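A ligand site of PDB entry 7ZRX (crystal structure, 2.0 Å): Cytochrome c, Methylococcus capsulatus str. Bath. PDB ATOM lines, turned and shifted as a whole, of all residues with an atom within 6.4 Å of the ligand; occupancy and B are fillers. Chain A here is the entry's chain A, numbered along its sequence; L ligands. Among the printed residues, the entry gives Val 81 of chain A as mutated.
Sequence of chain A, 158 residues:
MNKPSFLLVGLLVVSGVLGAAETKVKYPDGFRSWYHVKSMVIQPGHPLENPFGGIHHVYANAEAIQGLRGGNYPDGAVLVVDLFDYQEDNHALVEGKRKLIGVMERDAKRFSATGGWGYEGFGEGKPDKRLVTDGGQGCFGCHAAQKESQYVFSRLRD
Residues that only touch the ligand: Met 40 (3.5 Å), Leu 48 (3.7 Å), Phe 52 (3.7 Å), Val 58 (3.7 Å), Leu 79 (3.4 Å), Val 80 (3.97 Å), Val 81 (3.4 Å), Gly 102 (3.4 Å), Val 103 (3.7 Å), Met 104 (3.7 Å), Tyr 119 (3.99 Å), Glu 120 (3.1 Å), Val 132 (3.7 Å) and Val 152 (3.3 Å).
21 residues have an atom within 4 Å of the ligand: Lys 38, Met 40, Leu 48, Phe 52, His 56, Val 58, Leu 79, Val 80, Val 81, Gly 102, Val 103, Met 104, Tyr 119, Glu 120, Val 132, Cys 139, Cys 142, His 143, Val 152, Phe 153 and Ser 154.
The backbone carbonyl oxygen of Phe 153 lies within hydrogen-bond range of the guanidinium group of Arg 155 (3.2 Å).
The side-chain carboxylate (OE2) of Glu 120 is in hydrogen-bond range of the backbone NH (N) of Val 132, at 3.1 Å.
The backbone NH of Gly 102 lies within hydrogen-bond range of the backbone carbonyl oxygen of Val 81 (2.8 Å).
A ring nitrogen (ND1) of His 143 is in hydrogen-bond range of the backbone carbonyl oxygen of Tyr 151 (2.8 Å).
O of Glu 120 is in hydrogen-bond range of N of Val 103 (2.7 Å).
N of His 56 sits at hydrogen-bond distance from O of Met 40, at 2.9 Å.
The backbone NH of Tyr 59 lies within hydrogen-bond range of the backbone carbonyl oxygen of Val 80 (2.8 Å).
The backbone NH of Leu 131 is in hydrogen-bond range of the side-chain carboxylate of Glu 120.
A carbon (C25) of the ligand is bonded to the side-chain sulfur of Cys 142, at 1.8 Å.
A ring nitrogen (NE2) of His 56 is in hydrogen-bond range of an oxygen (O3) of the ligand, at 2.5 Å.
The backbone NH of Ser 154 is in hydrogen-bond range of an oxygen (O1) of the ligand (2.8 Å).
NZ of Lys 38 is in salt-bridge range of O4 of the ligand, at 2.6 Å.
A ring nitrogen (NE2) of His 143 binds an iron atom (FE1) of the ligand, 2.1 Å away.
The backbone NH (N) of Phe 153 is in hydrogen-bond range of an oxygen (O2) of the ligand, at 2.9 Å.
OG of Ser 154 lies within hydrogen-bond range of O1 of the ligand.
The side-chain sulfur (SG) of Cys 139 is bonded to a carbon (C18) of the ligand, at 1.7 Å.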
ATOM      1  N   LYS A  38       8.846  33.885  12.245  1.00  0.00           N
ATOM      2  CA  LYS A  38       7.731  32.953  11.985  1.00  0.00           C
ATOM      3  C   LYS A  38       8.193  31.531  12.309  1.00  0.00           C
ATOM      4  O   LYS A  38       9.433  31.278  12.502  1.00  0.00           O
ATOM      5  CB  LYS A  38       7.273  33.045  10.536  1.00  0.00           C
ATOM      6  CG  LYS A  38       8.268  32.558   9.493  1.00  0.00           C
ATOM      7  CD  LYS A  38       7.727  32.436   8.095  1.00  0.00           C
ATOM      8  CE  LYS A  38       6.493  31.567   8.017  1.00  0.00           C
ATOM      9  NZ  LYS A  38       6.239  31.190   6.622  1.00  0.00           N
ATOM     10  N   SER A  39       7.227  30.625  12.339  1.00  0.00           N
ATOM     11  CA  SER A  39       7.398  29.161  12.477  1.00  0.00           C
ATOM     12  C   SER A  39       6.488  28.466  11.470  1.00  0.00           C
ATOM     13  O   SER A  39       5.504  29.069  10.950  1.00  0.00           O
ATOM     14  CB  SER A  39       7.144  28.715  13.878  1.00  0.00           C
ATOM     15  OG  SER A  39       8.030  29.377  14.781  1.00  0.00           O
ATOM     16  N   MET A  40       6.823  27.209  11.219  1.00  0.00           N
ATOM     17  CA  MET A  40       6.083  26.249  10.381  1.00  0.00           C
ATOM     18  C   MET A  40       6.450  24.810  10.830  1.00  0.00           C
ATOM     19  O   MET A  40       7.578  24.613  11.407  1.00  0.00           O
ATOM     20  CB  MET A  40       6.453  26.462   8.900  1.00  0.00           C
ATOM     21  CG  MET A  40       5.550  25.664   7.941  1.00  0.00           C
ATOM     22  SD  MET A  40       6.126  25.833   6.243  1.00  0.00           S
ATOM     23  CE  MET A  40       5.683  27.547   5.945  1.00  0.00           C
ATOM     24  N   ILE A  42       6.716  20.977   9.127  1.00  0.00           N
ATOM     25  CA  ILE A  42       6.739  20.090   7.940  1.00  0.00           C
ATOM     26  C   ILE A  42       6.691  18.645   8.441  1.00  0.00           C
ATOM     27  O   ILE A  42       7.593  18.248   9.207  1.00  0.00           O
ATOM     28  CB  ILE A  42       7.953  20.405   7.071  1.00  0.00           C
ATOM     29  CG1 ILE A  42       7.804  21.808   6.471  1.00  0.00           C
ATOM     30  CG2 ILE A  42       8.183  19.333   6.018  1.00  0.00           C
ATOM     31  CD1 ILE A  42       9.000  22.262   5.667  1.00  0.00           C
ATOM     32  N   LEU A  48       8.922  18.313   1.008  1.00  0.00           N
ATOM     33  CA  LEU A  48      10.210  18.765   1.620  1.00  0.00           C
ATOM     34  C   LEU A  48      10.570  17.943   2.882  1.00  0.00           C
ATOM     35  O   LEU A  48      11.576  18.276   3.583  1.00  0.00           O
ATOM     36  CB  LEU A  48      10.098  20.278   1.890  1.00  0.00           C
ATOM     37  CG  LEU A  48      10.036  21.200   0.648  1.00  0.00           C
ATOM     38  CD1 LEU A  48      10.083  22.697   1.027  1.00  0.00           C
ATOM     39  CD2 LEU A  48      11.135  20.874  -0.361  1.00  0.00           C
ATOM     40  N   PHE A  52      13.902  18.689   5.396  1.00  0.00           N
ATOM     41  CA  PHE A  52      13.349  19.898   6.051  1.00  0.00           C
ATOM     42  C   PHE A  52      12.249  19.521   7.035  1.00  0.00           C
ATOM     43  O   PHE A  52      11.667  20.436   7.656  1.00  0.00           O
ATOM     44  CB  PHE A  52      12.892  20.879   4.968  1.00  0.00           C
ATOM     45  CG  PHE A  52      14.026  21.337   4.071  1.00  0.00           C
ATOM     46  CD1 PHE A  52      15.252  21.651   4.615  1.00  0.00           C
ATOM     47  CD2 PHE A  52      13.855  21.443   2.712  1.00  0.00           C
ATOM     48  CE1 PHE A  52      16.287  22.072   3.805  1.00  0.00           C
ATOM     49  CE2 PHE A  52      14.885  21.873   1.906  1.00  0.00           C
ATOM     50  CZ  PHE A  52      16.103  22.183   2.450  1.00  0.00           C
ATOM     51  N   HIS A  56      10.218  24.262  12.478  1.00  0.00           N
ATOM     52  CA  HIS A  56      11.278  25.263  12.209  1.00  0.00           C
ATOM     53  C   HIS A  56      10.818  26.664  12.618  1.00  0.00           C
ATOM     54  O   HIS A  56       9.612  26.976  12.536  1.00  0.00           O
ATOM     55  CB  HIS A  56      11.837  25.178  10.783  1.00  0.00           C
ATOM     56  CG  HIS A  56      10.956  25.700   9.720  1.00  0.00           C
ATOM     57  ND1 HIS A  56      10.440  24.883   8.761  1.00  0.00           N
ATOM     58  CD2 HIS A  56      10.585  26.956   9.402  1.00  0.00           C
ATOM     59  CE1 HIS A  56       9.772  25.613   7.887  1.00  0.00           C
ATOM     60  NE2 HIS A  56       9.854  26.869   8.257  1.00  0.00           N
ATOM     61  N   VAL A  58      12.086  30.697  12.244  1.00  0.00           N
ATOM     62  CA  VAL A  58      12.959  31.658  11.526  1.00  0.00           C
ATOM     63  C   VAL A  58      13.308  32.806  12.481  1.00  0.00           C
ATOM     64  O   VAL A  58      12.402  33.312  13.161  1.00  0.00           O
ATOM     65  CB  VAL A  58      12.316  32.138  10.217  1.00  0.00           C
ATOM     66  CG1 VAL A  58      13.271  33.060   9.455  1.00  0.00           C
ATOM     67  CG2 VAL A  58      11.873  30.988   9.328  1.00  0.00           C
ATOM     68  N   TYR A  59      14.584  33.204  12.510  1.00  0.00           N
ATOM     69  CA  TYR A  59      15.110  34.353  13.303  1.00  0.00           C
ATOM     70  C   TYR A  59      15.783  35.358  12.375  1.00  0.00           C
ATOM     71  O   TYR A  59      16.252  34.993  11.283  1.00  0.00           O
ATOM     72  CB  TYR A  59      16.087  33.862  14.365  1.00  0.00           C
ATOM     73  CG  TYR A  59      15.498  32.953  15.395  1.00  0.00           C
ATOM     74  CD1 TYR A  59      14.882  33.467  16.511  1.00  0.00           C
ATOM     75  CD2 TYR A  59      15.531  31.572  15.225  1.00  0.00           C
ATOM     76  CE1 TYR A  59      14.326  32.638  17.453  1.00  0.00           C
ATOM     77  CE2 TYR A  59      15.004  30.733  16.189  1.00  0.00           C
ATOM     78  CZ  TYR A  59      14.358  31.261  17.273  1.00  0.00           C
ATOM     79  OH  TYR A  59      13.852  30.446  18.230  1.00  0.00           O
ATOM     80  N   LEU A  79      19.662  35.758   8.404  1.00  0.00           N
ATOM     81  CA  LEU A  79      18.438  34.964   8.687  1.00  0.00           C
ATOM     82  C   LEU A  79      18.883  33.561   9.055  1.00  0.00           C
ATOM     83  O   LEU A  79      19.864  33.024   8.466  1.00  0.00           O
ATOM     84  CB  LEU A  79      17.579  34.946   7.424  1.00  0.00           C
ATOM     85  CG  LEU A  79      17.017  36.334   7.024  1.00  0.00           C
ATOM     86  CD1 LEU A  79      16.609  36.346   5.567  1.00  0.00           C
ATOM     87  CD2 LEU A  79      15.835  36.701   7.893  1.00  0.00           C
ATOM     88  N   VAL A  80      18.240  33.018  10.066  1.00  0.00           N
ATOM     89  CA  VAL A  80      18.508  31.653  10.544  1.00  0.00           C
ATOM     90  C   VAL A  80      17.196  30.885  10.509  1.00  0.00           C
ATOM     91  O   VAL A  80      16.199  31.362  11.113  1.00  0.00           O
ATOM     92  CB  VAL A  80      19.123  31.668  11.962  1.00  0.00           C
ATOM     93  CG1 VAL A  80      19.321  30.243  12.477  1.00  0.00           C
ATOM     94  CG2 VAL A  80      20.422  32.441  12.001  1.00  0.00           C
ATOM     95  N   VAL A  81      17.231  29.683   9.957  1.00  0.00           N
ATOM     96  CA  VAL A  81      16.114  28.720  10.143  1.00  0.00           C
ATOM     97  C   VAL A  81      16.574  27.596  11.076  1.00  0.00           C
ATOM     98  O   VAL A  81      17.622  26.961  10.807  1.00  0.00           O
ATOM     99  CB  VAL A  81      15.505  28.280   8.798  1.00  0.00           C
ATOM    100  CG1 VAL A  81      16.544  27.648   7.878  1.00  0.00           C
ATOM    101  CG2 VAL A  81      14.293  27.382   9.009  1.00  0.00           C
ATOM    102  N   ILE A 101      20.664  24.032  11.719  1.00  0.00           N
ATOM    103  CA  ILE A 101      20.204  25.405  11.399  1.00  0.00           C
ATOM    104  C   ILE A 101      20.643  25.664   9.962  1.00  0.00           C
ATOM    105  O   ILE A 101      21.674  25.090   9.522  1.00  0.00           O
ATOM    106  CB  ILE A 101      20.713  26.455  12.411  1.00  0.00           C
ATOM    107  CG1 ILE A 101      22.228  26.663  12.336  1.00  0.00           C
ATOM    108  CG2 ILE A 101      20.251  26.124  13.827  1.00  0.00           C
ATOM    109  CD1 ILE A 101      22.788  27.695  13.308  1.00  0.00           C
ATOM    110  N   GLY A 102      19.812  26.404   9.217  1.00  0.00           N
ATOM    111  CA  GLY A 102      20.219  27.011   7.947  1.00  0.00           C
ATOM    112  C   GLY A 102      20.486  28.490   8.169  1.00  0.00           C
ATOM    113  O   GLY A 102      19.800  29.091   9.006  1.00  0.00           O
ATOM    114  N   VAL A 103      21.418  29.064   7.417  1.00  0.00           N
ATOM    115  CA  VAL A 103      21.894  30.454   7.644  1.00  0.00           C
ATOM    116  C   VAL A 103      22.047  31.118   6.291  1.00  0.00           C
ATOM    117  O   VAL A 103      22.689  30.504   5.362  1.00  0.00           O
ATOM    118  CB  VAL A 103      23.214  30.512   8.444  1.00  0.00           C
ATOM    119  CG1 VAL A 103      23.587  31.952   8.823  1.00  0.00           C
ATOM    120  CG2 VAL A 103      23.129  29.644   9.686  1.00  0.00           C
ATOM    121  N   MET A 104      21.491  32.326   6.206  1.00  0.00           N
ATOM    122  CA  MET A 104      21.727  33.191   5.037  1.00  0.00           C
ATOM    123  C   MET A 104      22.363  34.468   5.557  1.00  0.00           C
ATOM    124  O   MET A 104      21.809  35.065   6.503  1.00  0.00           O
ATOM    125  CB  MET A 104      20.438  33.518   4.283  1.00  0.00           C
ATOM    126  CG  MET A 104      19.872  32.363   3.518  1.00  0.00           C
ATOM    127  SD  MET A 104      18.100  32.656   3.116  1.00  0.00           S
ATOM    128  CE  MET A 104      18.240  33.815   1.760  1.00  0.00           C
ATOM    129  N   GLY A 118      25.102  34.496   1.272  1.00  0.00           N
ATOM    130  CA  GLY A 118      25.868  33.276   1.608  1.00  0.00           C
ATOM    131  C   GLY A 118      24.960  32.265   2.273  1.00  0.00           C
ATOM    132  O   GLY A 118      24.313  32.616   3.250  1.00  0.00           O
ATOM    133  N   TYR A 119      24.928  31.024   1.766  1.00  0.00           N
ATOM    134  CA  TYR A 119      24.108  29.928   2.314  1.00  0.00           C
ATOM    135  C   TYR A 119      25.016  28.933   3.068  1.00  0.00           C
ATOM    136  O   TYR A 119      25.935  28.409   2.465  1.00  0.00           O
ATOM    137  CB  TYR A 119      23.320  29.307   1.163  1.00  0.00           C
ATOM    138  CG  TYR A 119      22.265  30.187   0.543  1.00  0.00           C
ATOM    139  CD1 TYR A 119      22.555  31.046  -0.511  1.00  0.00           C
ATOM    140  CD2 TYR A 119      20.940  30.112   0.948  1.00  0.00           C
ATOM    141  CE1 TYR A 119      21.574  31.818  -1.111  1.00  0.00           C
ATOM    142  CE2 TYR A 119      19.958  30.890   0.360  1.00  0.00           C
ATOM    143  CZ  TYR A 119      20.271  31.752  -0.654  1.00  0.00           C
ATOM    144  OH  TYR A 119      19.305  32.524  -1.214  1.00  0.00           O
ATOM    145  N   GLU A 120      24.684  28.608   4.314  1.00  0.00           N
ATOM    146  CA  GLU A 120      25.354  27.536   5.108  1.00  0.00           C
ATOM    147  C   GLU A 120      24.345  26.814   5.999  1.00  0.00           C
ATOM    148  O   GLU A 120      23.326  27.424   6.373  1.00  0.00           O
ATOM    149  CB  GLU A 120      26.470  28.151   5.972  1.00  0.00           C
ATOM    150  CG  GLU A 120      27.317  27.148   6.760  1.00  0.00           C
ATOM    151  CD  GLU A 120      28.171  26.257   5.887  1.00  0.00           C
ATOM    152  OE1 GLU A 120      29.365  26.586   5.681  1.00  0.00           O
ATOM    153  OE2 GLU A 120      27.642  25.230   5.443  1.00  0.00           O
ATOM    154  N   GLY A 121      24.641  25.550   6.288  1.00  0.00           N
ATOM    155  CA  GLY A 121      23.940  24.703   7.258  1.00  0.00           C
ATOM    156  C   GLY A 121      24.907  24.258   8.339  1.00  0.00           C
ATOM    157  O   GLY A 121      26.130  24.048   8.041  1.00  0.00           O
ATOM    158  N   LEU A 131      27.700  22.149   6.569  1.00  0.00           N
ATOM    159  CA  LEU A 131      27.014  21.103   5.763  1.00  0.00           C
ATOM    160  C   LEU A 131      27.155  21.375   4.270  1.00  0.00           C
ATOM    161  O   LEU A 131      27.052  20.418   3.545  1.00  0.00           O
ATOM    162  CB  LEU A 131      25.534  20.974   6.109  1.00  0.00           C
ATOM    163  CG  LEU A 131      25.232  20.568   7.558  1.00  0.00           C
ATOM    164  CD1 LEU A 131      23.730  20.707   7.820  1.00  0.00           C
ATOM    165  CD2 LEU A 131      25.721  19.152   7.845  1.00  0.00           C
ATOM    166  N   VAL A 132      27.327  22.617   3.863  1.00  0.00           N
ATOM    167  CA  VAL A 132      27.169  22.968   2.426  1.00  0.00           C
ATOM    168  C   VAL A 132      28.489  22.683   1.717  1.00  0.00           C
ATOM    169  O   VAL A 132      29.536  23.136   2.201  1.00  0.00           O
ATOM    170  CB  VAL A 132      26.701  24.420   2.234  1.00  0.00           C
ATOM    171  CG1 VAL A 132      26.969  24.855   0.793  1.00  0.00           C
ATOM    172  CG2 VAL A 132      25.218  24.585   2.611  1.00  0.00           C
ATOM    173  N   GLY A 136      26.713  26.748  -2.002  1.00  0.00           N
ATOM    174  CA  GLY A 136      25.340  27.244  -1.771  1.00  0.00           C
ATOM    175  C   GLY A 136      24.482  27.247  -3.027  1.00  0.00           C
ATOM    176  O   GLY A 136      23.345  27.717  -2.949  1.00  0.00           O
ATOM    177  N   GLY A 138      22.969  24.689  -4.567  1.00  0.00           N
ATOM    178  CA  GLY A 138      21.755  23.928  -4.219  1.00  0.00           C
ATOM    179  C   GLY A 138      20.737  24.797  -3.480  1.00  0.00           C
ATOM    180  O   GLY A 138      19.561  24.837  -3.896  1.00  0.00           O
ATOM    181  N   CYS A 139      21.160  25.495  -2.433  1.00  0.00           N
ATOM    182  CA  CYS A 139      20.274  26.376  -1.622  1.00  0.00           C
ATOM    183  C   CYS A 139      19.684  27.447  -2.565  1.00  0.00           C
ATOM    184  O   CYS A 139      18.430  27.706  -2.579  1.00  0.00           O
ATOM    185  CB  CYS A 139      21.049  27.045  -0.483  1.00  0.00           C
ATOM    186  SG  CYS A 139      21.964  25.906   0.533  1.00  0.00           S
ATOM    187  N   PHE A 140      20.566  28.110  -3.274  1.00  0.00           N
ATOM    188  CA  PHE A 140      20.225  29.277  -4.110  1.00  0.00           C
ATOM    189  C   PHE A 140      19.236  28.832  -5.193  1.00  0.00           C
ATOM    190  O   PHE A 140      18.330  29.607  -5.473  1.00  0.00           O
ATOM    191  CB  PHE A 140      21.514  29.877  -4.654  1.00  0.00           C
ATOM    192  CG  PHE A 140      21.331  31.050  -5.581  1.00  0.00           C
ATOM    193  CD1 PHE A 140      20.557  32.125  -5.205  1.00  0.00           C
ATOM    194  CD2 PHE A 140      21.951  31.071  -6.820  1.00  0.00           C
ATOM    195  CE1 PHE A 140      20.405  33.223  -6.046  1.00  0.00           C
ATOM    196  CE2 PHE A 140      21.789  32.164  -7.660  1.00  0.00           C
ATOM    197  CZ  PHE A 140      21.020  33.233  -7.266  1.00  0.00           C
ATOM    198  N   GLY A 141      19.397  27.621  -5.757  1.00  0.00           N
ATOM    199  CA  GLY A 141      18.510  27.039  -6.783  1.00  0.00           C
ATOM    200  C   GLY A 141      17.046  27.122  -6.364  1.00  0.00           C
ATOM    201  O   GLY A 141      16.216  27.450  -7.194  1.00  0.00           O
ATOM    202  N   CYS A 142      16.722  26.876  -5.102  1.00  0.00           N
ATOM    203  CA  CYS A 142      15.323  26.900  -4.623  1.00  0.00           C
ATOM    204  C   CYS A 142      14.960  28.344  -4.265  1.00  0.00           C
ATOM    205  O   CYS A 142      13.869  28.796  -4.639  1.00  0.00           O
ATOM    206  CB  CYS A 142      15.151  25.946  -3.457  1.00  0.00           C
ATOM    207  SG  CYS A 142      13.477  25.738  -2.920  1.00  0.00           S
ATOM    208  N   HIS A 143      15.860  29.062  -3.596  1.00  0.00           N
ATOM    209  CA  HIS A 143      15.599  30.429  -3.104  1.00  0.00           C
ATOM    210  C   HIS A 143      15.427  31.400  -4.302  1.00  0.00           C
ATOM    211  O   HIS A 143      14.824  32.491  -4.103  1.00  0.00           O
ATOM    212  CB  HIS A 143      16.675  30.848  -2.062  1.00  0.00           C
ATOM    213  CG  HIS A 143      16.393  30.318  -0.684  1.00  0.00           C
ATOM    214  ND1 HIS A 143      15.957  31.121   0.341  1.00  0.00           N
ATOM    215  CD2 HIS A 143      16.444  29.065  -0.170  1.00  0.00           C
ATOM    216  CE1 HIS A 143      15.786  30.366   1.437  1.00  0.00           C
ATOM    217  NE2 HIS A 143      16.052  29.109   1.148  1.00  0.00           N
ATOM    218  N   TYR A 151      15.223  36.860  -2.407  1.00  0.00           N
ATOM    219  CA  TYR A 151      15.541  35.423  -2.185  1.00  0.00           C
ATOM    220  C   TYR A 151      15.153  34.957  -0.792  1.00  0.00           C
ATOM    221  O   TYR A 151      15.646  33.852  -0.404  1.00  0.00           O
ATOM    222  CB  TYR A 151      17.023  35.162  -2.433  1.00  0.00           C
ATOM    223  CG  TYR A 151      17.471  35.624  -3.787  1.00  0.00           C
ATOM    224  CD1 TYR A 151      17.087  34.949  -4.922  1.00  0.00           C
ATOM    225  CD2 TYR A 151      18.236  36.776  -3.921  1.00  0.00           C
ATOM    226  CE1 TYR A 151      17.475  35.364  -6.181  1.00  0.00           C
ATOM    227  CE2 TYR A 151      18.657  37.192  -5.177  1.00  0.00           C
ATOM    228  CZ  TYR A 151      18.279  36.480  -6.304  1.00  0.00           C
ATOM    229  OH  TYR A 151      18.674  36.885  -7.536  1.00  0.00           O
ATOM    230  N   VAL A 152      14.271  35.692  -0.122  1.00  0.00           N
ATOM    231  CA  VAL A 152      13.692  35.339   1.205  1.00  0.00           C
ATOM    232  C   VAL A 152      12.235  34.886   1.068  1.00  0.00           C
ATOM    233  O   VAL A 152      11.426  35.656   0.536  1.00  0.00           O
ATOM    234  CB  VAL A 152      13.811  36.527   2.163  1.00  0.00           C
ATOM    235  CG1 VAL A 152      13.190  36.194   3.507  1.00  0.00           C
ATOM    236  CG2 VAL A 152      15.271  36.969   2.273  1.00  0.00           C
ATOM    237  N   PHE A 153      11.901  33.691   1.553  1.00  0.00           N
ATOM    238  CA  PHE A 153      10.542  33.121   1.558  1.00  0.00           C
ATOM    239  C   PHE A 153       9.722  33.786   2.667  1.00  0.00           C
ATOM    240  O   PHE A 153       8.569  34.153   2.440  1.00  0.00           O
ATOM    241  CB  PHE A 153      10.586  31.606   1.761  1.00  0.00           C
ATOM    242  CG  PHE A 153      11.028  30.815   0.564  1.00  0.00           C
ATOM    243  CD1 PHE A 153      12.338  30.350   0.436  1.00  0.00           C
ATOM    244  CD2 PHE A 153      10.111  30.509  -0.442  1.00  0.00           C
ATOM    245  CE1 PHE A 153      12.732  29.602  -0.669  1.00  0.00           C
ATOM    246  CE2 PHE A 153      10.497  29.757  -1.546  1.00  0.00           C
ATOM    247  CZ  PHE A 153      11.805  29.297  -1.662  1.00  0.00           C
ATOM    248  N   SER A 154      10.294  33.910   3.863  1.00  0.00           N
ATOM    249  CA  SER A 154       9.599  34.305   5.107  1.00  0.00           C
ATOM    250  C   SER A 154       9.042  35.718   4.965  1.00  0.00           C
ATOM    251  O   SER A 154       9.729  36.573   4.372  1.00  0.00           O
ATOM    252  CB  SER A 154      10.514  34.196   6.311  1.00  0.00           C
ATOM    253  OG  SER A 154      10.868  32.855   6.591  1.00  0.00           O
ATOM    254  N   ARG A 155       7.835  35.952   5.508  1.00  0.00           N
ATOM    255  CA  ARG A 155       7.205  37.296   5.621  1.00  0.00           C
ATOM    256  C   ARG A 155       7.055  37.649   7.092  1.00  0.00           C
ATOM    257  O   ARG A 155       6.635  36.797   7.906  1.00  0.00           O
ATOM    258  CB  ARG A 155       5.817  37.354   4.967  1.00  0.00           C
ATOM    259  CG  ARG A 155       5.811  36.913   3.512  1.00  0.00           C
ATOM    260  CD  ARG A 155       6.568  37.861   2.610  1.00  0.00           C
ATOM    261  NE  ARG A 155       6.602  37.258   1.283  1.00  0.00           N
ATOM    262  CZ  ARG A 155       7.695  36.854   0.639  1.00  0.00           C
ATOM    263  NH1 ARG A 155       8.906  37.010   1.151  1.00  0.00           N
ATOM    264  NH2 ARG A 155       7.555  36.287  -0.546  1.00  0.00           N
HETATM  265 FE1  LIG L   1      15.764  27.518   2.524  1.00  0.00          FE
HETATM  266  C1  LIG L   1      13.676  29.380   4.475  1.00  0.00           C
HETATM  267  C2  LIG L   1      18.497  28.619   4.370  1.00  0.00           C
HETATM  268  C3  LIG L   1      17.749  25.234   0.869  1.00  0.00           C
HETATM  269  C4  LIG L   1      13.067  26.460   0.696  1.00  0.00           C
HETATM  270  N1  LIG L   1      16.077  28.782   4.139  1.00  0.00           N
HETATM  271  C5  LIG L   1      15.115  29.497   4.777  1.00  0.00           C
HETATM  272  C6  LIG L   1      15.611  30.413   5.809  1.00  0.00           C
HETATM  273  C7  LIG L   1      17.061  30.224   5.759  1.00  0.00           C
HETATM  274  C8  LIG L   1      17.212  29.204   4.722  1.00  0.00           C
HETATM  275  C9  LIG L   1      18.050  30.873   6.632  1.00  0.00           C
HETATM  276  C10 LIG L   1      14.802  31.383   6.580  1.00  0.00           C
HETATM  277  C11 LIG L   1      14.758  32.609   5.619  1.00  0.00           C
HETATM  278  C12 LIG L   1      13.718  32.611   4.448  1.00  0.00           C
HETATM  279  O1  LIG L   1      12.516  32.471   4.724  1.00  0.00           O
HETATM  280  O2  LIG L   1      14.066  32.717   3.228  1.00  0.00           O
HETATM  281  N2  LIG L   1      17.767  26.995   2.592  1.00  0.00           N
HETATM  282  C13 LIG L   1      18.692  27.498   3.439  1.00  0.00           C
HETATM  283  C14 LIG L   1      20.052  26.963   3.230  1.00  0.00           C
HETATM  284  C15 LIG L   1      19.843  25.931   2.208  1.00  0.00           C
HETATM  285  C16 LIG L   1      18.387  26.040   1.915  1.00  0.00           C
HETATM  286  C17 LIG L   1      21.258  27.352   4.002  1.00  0.00           C
HETATM  287  C18 LIG L   1      20.900  25.021   1.596  1.00  0.00           C
HETATM  288  C19 LIG L   1      21.518  24.085   2.583  1.00  0.00           C
HETATM  289  N3  LIG L   1      15.438  26.112   1.046  1.00  0.00           N
HETATM  290  C20 LIG L   1      16.361  25.323   0.455  1.00  0.00           C
HETATM  291  C21 LIG L   1      15.876  24.511  -0.662  1.00  0.00           C
HETATM  292  C22 LIG L   1      14.450  24.851  -0.682  1.00  0.00           C
HETATM  293  C23 LIG L   1      14.333  25.871   0.358  1.00  0.00           C
HETATM  294  C24 LIG L   1      16.686  23.541  -1.433  1.00  0.00           C
HETATM  295  C25 LIG L   1      13.423  24.427  -1.694  1.00  0.00           C
HETATM  296  C26 LIG L   1      13.411  23.035  -2.315  1.00  0.00           C
HETATM  297  N4  LIG L   1      13.717  27.827   2.617  1.00  0.00           N
HETATM  298  C27 LIG L   1      12.775  27.300   1.831  1.00  0.00           C
HETATM  299  C28 LIG L   1      11.394  27.683   2.143  1.00  0.00           C
HETATM  300  C29 LIG L   1      11.546  28.546   3.291  1.00  0.00           C
HETATM  301  C30 LIG L   1      13.024  28.541   3.486  1.00  0.00           C
HETATM  302  C31 LIG L   1      10.153  27.263   1.455  1.00  0.00           C
HETATM  303  C32 LIG L   1      10.451  29.249   4.032  1.00  0.00           C
HETATM  304  C33 LIG L   1      10.048  28.441   5.251  1.00  0.00           C
HETATM  305  C34 LIG L   1       8.957  29.121   6.070  1.00  0.00           C
HETATM  306  O3  LIG L   1       8.680  28.814   7.255  1.00  0.00           O
HETATM  307  O4  LIG L   1       8.312  30.031   5.495  1.00  0.00           O
